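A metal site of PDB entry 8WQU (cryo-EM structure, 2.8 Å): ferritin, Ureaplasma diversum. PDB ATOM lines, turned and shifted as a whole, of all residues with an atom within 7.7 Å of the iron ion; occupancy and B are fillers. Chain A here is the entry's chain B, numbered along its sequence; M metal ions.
The iron ion is bound by NE2 of His 65 (2.1 Å), OD2 of Asp 60 (2.1 Å), OD2 of Asp 138 (2.4 Å) and OD2 of Asp 142 (2.4 Å).
The iron ion has four donor atoms within binding distance.
The nearest printed residue that does not touch the iron ion is Lys 61 (4.5 Å).
The backbone carbonyl oxygen (O) of His 65 lies within hydrogen-bond range of the side-chain hydroxyl (OH) of Tyr 135 (3.2 Å).
O of His 65 sits at hydrogen-bond distance from ND2 of Asn 27.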
ATOM      1  N   ASN A  27     -15.325   3.072 -13.375  1.00  0.00           N
ATOM      2  CA  ASN A  27     -14.730   2.004 -12.585  1.00  0.00           C
ATOM      3  C   ASN A  27     -13.867   1.096 -13.440  1.00  0.00           C
ATOM      4  O   ASN A  27     -12.736   0.750 -13.055  1.00  0.00           O
ATOM      5  CB  ASN A  27     -15.813   1.206 -11.874  1.00  0.00           C
ATOM      6  CG  ASN A  27     -16.105   1.736 -10.496  1.00  0.00           C
ATOM      7  OD1 ASN A  27     -15.234   2.310  -9.850  1.00  0.00           O
ATOM      8  ND2 ASN A  27     -17.334   1.551 -10.040  1.00  0.00           N
ATOM      9  N   HIS A  56      -4.038  -4.665  -5.518  1.00  0.00           N
ATOM     10  CA  HIS A  56      -5.237  -4.917  -4.729  1.00  0.00           C
ATOM     11  C   HIS A  56      -6.324  -3.897  -5.040  1.00  0.00           C
ATOM     12  O   HIS A  56      -7.493  -4.246  -5.191  1.00  0.00           O
ATOM     13  CB  HIS A  56      -4.890  -4.914  -3.243  1.00  0.00           C
ATOM     14  CG  HIS A  56      -6.062  -5.189  -2.353  1.00  0.00           C
ATOM     15  ND1 HIS A  56      -7.010  -6.147  -2.636  1.00  0.00           N
ATOM     16  CD2 HIS A  56      -6.428  -4.635  -1.176  1.00  0.00           C
ATOM     17  CE1 HIS A  56      -7.913  -6.170  -1.675  1.00  0.00           C
ATOM     18  NE2 HIS A  56      -7.579  -5.259  -0.771  1.00  0.00           N
ATOM     19  N   LEU A  57      -5.931  -2.620  -5.154  1.00  0.00           N
ATOM     20  CA  LEU A  57      -6.899  -1.595  -5.556  1.00  0.00           C
ATOM     21  C   LEU A  57      -7.508  -1.907  -6.921  1.00  0.00           C
ATOM     22  O   LEU A  57      -8.726  -1.764  -7.106  1.00  0.00           O
ATOM     23  CB  LEU A  57      -6.237  -0.225  -5.595  1.00  0.00           C
ATOM     24  CG  LEU A  57      -5.699   0.417  -4.320  1.00  0.00           C
ATOM     25  CD1 LEU A  57      -5.236   1.817  -4.645  1.00  0.00           C
ATOM     26  CD2 LEU A  57      -6.760   0.433  -3.248  1.00  0.00           C
ATOM     27  N   ASP A  60     -10.013  -4.717  -6.718  1.00  0.00           N
ATOM     28  CA  ASP A  60     -11.201  -4.177  -6.071  1.00  0.00           C
ATOM     29  C   ASP A  60     -12.094  -3.447  -7.071  1.00  0.00           C
ATOM     30  O   ASP A  60     -13.297  -3.685  -7.135  1.00  0.00           O
ATOM     31  CB  ASP A  60     -10.792  -3.255  -4.926  1.00  0.00           C
ATOM     32  CG  ASP A  60     -11.918  -2.979  -3.957  1.00  0.00           C
ATOM     33  OD1 ASP A  60     -12.505  -3.947  -3.454  1.00  0.00           O
ATOM     34  OD2 ASP A  60     -12.196  -1.787  -3.696  1.00  0.00           O
ATOM     35  N   LYS A  61     -11.502  -2.543  -7.851  1.00  0.00           N
ATOM     36  CA  LYS A  61     -12.306  -1.735  -8.767  1.00  0.00           C
ATOM     37  C   LYS A  61     -12.901  -2.575  -9.886  1.00  0.00           C
ATOM     38  O   LYS A  61     -14.057  -2.375 -10.274  1.00  0.00           O
ATOM     39  CB  LYS A  61     -11.477  -0.605  -9.349  1.00  0.00           C
ATOM     40  CG  LYS A  61     -10.944   0.357  -8.329  1.00  0.00           C
ATOM     41  CD  LYS A  61     -12.029   1.260  -7.810  1.00  0.00           C
ATOM     42  CE  LYS A  61     -11.528   2.100  -6.653  1.00  0.00           C
ATOM     43  NZ  LYS A  61     -12.573   3.000  -6.137  1.00  0.00           N
ATOM     44  N   VAL A  64     -16.148  -6.133  -7.548  1.00  0.00           N
ATOM     45  CA  VAL A  64     -17.467  -5.923  -6.966  1.00  0.00           C
ATOM     46  C   VAL A  64     -18.043  -4.560  -7.318  1.00  0.00           C
ATOM     47  O   VAL A  64     -19.267  -4.393  -7.399  1.00  0.00           O
ATOM     48  CB  VAL A  64     -17.419  -6.144  -5.444  1.00  0.00           C
ATOM     49  CG1 VAL A  64     -16.978  -7.553  -5.130  1.00  0.00           C
ATOM     50  CG2 VAL A  64     -16.502  -5.141  -4.796  1.00  0.00           C
ATOM     51  N   HIS A  65     -17.191  -3.555  -7.569  1.00  0.00           N
ATOM     52  CA  HIS A  65     -17.677  -2.210  -7.826  1.00  0.00           C
ATOM     53  C   HIS A  65     -18.522  -2.112  -9.088  1.00  0.00           C
ATOM     54  O   HIS A  65     -19.309  -1.183  -9.212  1.00  0.00           O
ATOM     55  CB  HIS A  65     -16.524  -1.228  -7.906  1.00  0.00           C
ATOM     56  CG  HIS A  65     -15.973  -0.812  -6.573  1.00  0.00           C
ATOM     57  ND1 HIS A  65     -16.005   0.482  -6.136  1.00  0.00           N
ATOM     58  CD2 HIS A  65     -15.380  -1.539  -5.603  1.00  0.00           C
ATOM     59  CE1 HIS A  65     -15.452   0.546  -4.935  1.00  0.00           C
ATOM     60  NE2 HIS A  65     -15.072  -0.664  -4.590  1.00  0.00           N
ATOM     61  N   GLU A 106      -8.942   8.789  -6.388  1.00  0.00           N
ATOM     62  CA  GLU A 106      -9.928   8.417  -5.369  1.00  0.00           C
ATOM     63  C   GLU A 106     -10.753   9.629  -4.934  1.00  0.00           C
ATOM     64  O   GLU A 106     -11.978   9.545  -4.746  1.00  0.00           O
ATOM     65  CB  GLU A 106      -9.224   7.787  -4.170  1.00  0.00           C
ATOM     66  CG  GLU A 106      -8.582   6.459  -4.487  1.00  0.00           C
ATOM     67  CD  GLU A 106      -9.601   5.393  -4.834  1.00  0.00           C
ATOM     68  OE1 GLU A 106     -10.669   5.367  -4.198  1.00  0.00           O
ATOM     69  OE2 GLU A 106      -9.345   4.595  -5.753  1.00  0.00           O
ATOM     70  N   TRP A 134     -23.838   2.363  -0.044  1.00  0.00           N
ATOM     71  CA  TRP A 134     -22.641   1.527  -0.024  1.00  0.00           C
ATOM     72  C   TRP A 134     -21.441   2.243  -0.630  1.00  0.00           C
ATOM     73  O   TRP A 134     -20.340   2.225  -0.085  1.00  0.00           O
ATOM     74  CB  TRP A 134     -22.908   0.215  -0.760  1.00  0.00           C
ATOM     75  CG  TRP A 134     -21.862  -0.829  -0.534  1.00  0.00           C
ATOM     76  CD1 TRP A 134     -21.826  -1.733   0.470  1.00  0.00           C
ATOM     77  CD2 TRP A 134     -20.693  -1.068  -1.333  1.00  0.00           C
ATOM     78  NE1 TRP A 134     -20.719  -2.524   0.363  1.00  0.00           N
ATOM     79  CE2 TRP A 134     -20.003  -2.135  -0.739  1.00  0.00           C
ATOM     80  CE3 TRP A 134     -20.173  -0.490  -2.484  1.00  0.00           C
ATOM     81  CZ2 TRP A 134     -18.817  -2.634  -1.258  1.00  0.00           C
ATOM     82  CZ3 TRP A 134     -18.994  -0.983  -2.998  1.00  0.00           C
ATOM     83  CH2 TRP A 134     -18.328  -2.041  -2.387  1.00  0.00           C
ATOM     84  N   TYR A 135     -21.661   2.878  -1.777  1.00  0.00           N
ATOM     85  CA  TYR A 135     -20.574   3.589  -2.442  1.00  0.00           C
ATOM     86  C   TYR A 135     -20.189   4.845  -1.671  1.00  0.00           C
ATOM     87  O   TYR A 135     -19.005   5.188  -1.591  1.00  0.00           O
ATOM     88  CB  TYR A 135     -20.993   3.923  -3.871  1.00  0.00           C
ATOM     89  CG  TYR A 135     -21.151   2.700  -4.729  1.00  0.00           C
ATOM     90  CD1 TYR A 135     -22.312   1.947  -4.685  1.00  0.00           C
ATOM     91  CD2 TYR A 135     -20.141   2.269  -5.569  1.00  0.00           C
ATOM     92  CE1 TYR A 135     -22.463   0.822  -5.449  1.00  0.00           C
ATOM     93  CE2 TYR A 135     -20.281   1.146  -6.340  1.00  0.00           C
ATOM     94  CZ  TYR A 135     -21.440   0.434  -6.280  1.00  0.00           C
ATOM     95  OH  TYR A 135     -21.591  -0.691  -7.045  1.00  0.00           O
ATOM     96  N   ASP A 138     -17.860   3.394   1.007  1.00  0.00           N
ATOM     97  CA  ASP A 138     -16.606   2.804   0.540  1.00  0.00           C
ATOM     98  C   ASP A 138     -15.669   3.854  -0.029  1.00  0.00           C
ATOM     99  O   ASP A 138     -14.452   3.661  -0.007  1.00  0.00           O
ATOM    100  CB  ASP A 138     -16.887   1.711  -0.484  1.00  0.00           C
ATOM    101  CG  ASP A 138     -15.745   0.736  -0.591  1.00  0.00           C
ATOM    102  OD1 ASP A 138     -15.577  -0.098   0.321  1.00  0.00           O
ATOM    103  OD2 ASP A 138     -15.015   0.784  -1.603  1.00  0.00           O
ATOM    104  N   GLY A 139     -16.209   4.964  -0.522  1.00  0.00           N
ATOM    105  CA  GLY A 139     -15.336   6.039  -0.984  1.00  0.00           C
ATOM    106  C   GLY A 139     -14.415   6.543   0.102  1.00  0.00           C
ATOM    107  O   GLY A 139     -13.200   6.588  -0.073  1.00  0.00           O
ATOM    108  N   LYS A 141     -13.706   5.071   2.927  1.00  0.00           N
ATOM    109  CA  LYS A 141     -12.824   3.994   3.379  1.00  0.00           C
ATOM    110  C   LYS A 141     -11.574   3.876   2.505  1.00  0.00           C
ATOM    111  O   LYS A 141     -10.447   3.854   3.009  1.00  0.00           O
ATOM    112  CB  LYS A 141     -13.587   2.676   3.408  1.00  0.00           C
ATOM    113  CG  LYS A 141     -12.711   1.478   3.654  1.00  0.00           C
ATOM    114  CD  LYS A 141     -13.529   0.265   3.988  1.00  0.00           C
ATOM    115  CE  LYS A 141     -12.669  -0.876   4.506  1.00  0.00           C
ATOM    116  NZ  LYS A 141     -13.494  -2.034   4.925  1.00  0.00           N
ATOM    117  N   ASP A 142     -11.767   3.796   1.184  1.00  0.00           N
ATOM    118  CA  ASP A 142     -10.632   3.600   0.292  1.00  0.00           C
ATOM    119  C   ASP A 142      -9.717   4.811   0.281  1.00  0.00           C
ATOM    120  O   ASP A 142      -8.489   4.667   0.241  1.00  0.00           O
ATOM    121  CB  ASP A 142     -11.123   3.283  -1.116  1.00  0.00           C
ATOM    122  CG  ASP A 142     -11.701   1.897  -1.231  1.00  0.00           C
ATOM    123  OD1 ASP A 142     -11.384   1.044  -0.385  1.00  0.00           O
ATOM    124  OD2 ASP A 142     -12.478   1.652  -2.174  1.00  0.00           O
ATOM    125  N   GLU A 145      -7.504   4.588   3.444  1.00  0.00           N
ATOM    126  CA  GLU A 145      -6.411   3.618   3.407  1.00  0.00           C
ATOM    127  C   GLU A 145      -5.390   3.933   2.321  1.00  0.00           C
ATOM    128  O   GLU A 145      -4.293   3.377   2.349  1.00  0.00           O
ATOM    129  CB  GLU A 145      -6.950   2.202   3.237  1.00  0.00           C
ATOM    130  CG  GLU A 145      -7.604   1.921   1.918  1.00  0.00           C
ATOM    131  CD  GLU A 145      -8.088   0.489   1.818  1.00  0.00           C
ATOM    132  OE1 GLU A 145      -8.469   0.058   0.720  1.00  0.00           O
ATOM    133  OE2 GLU A 145      -8.080  -0.200   2.856  1.00  0.00           O
HETATM  134 FE    FE M   1     -13.586  -0.232  -3.201  1.00  0.00          FE
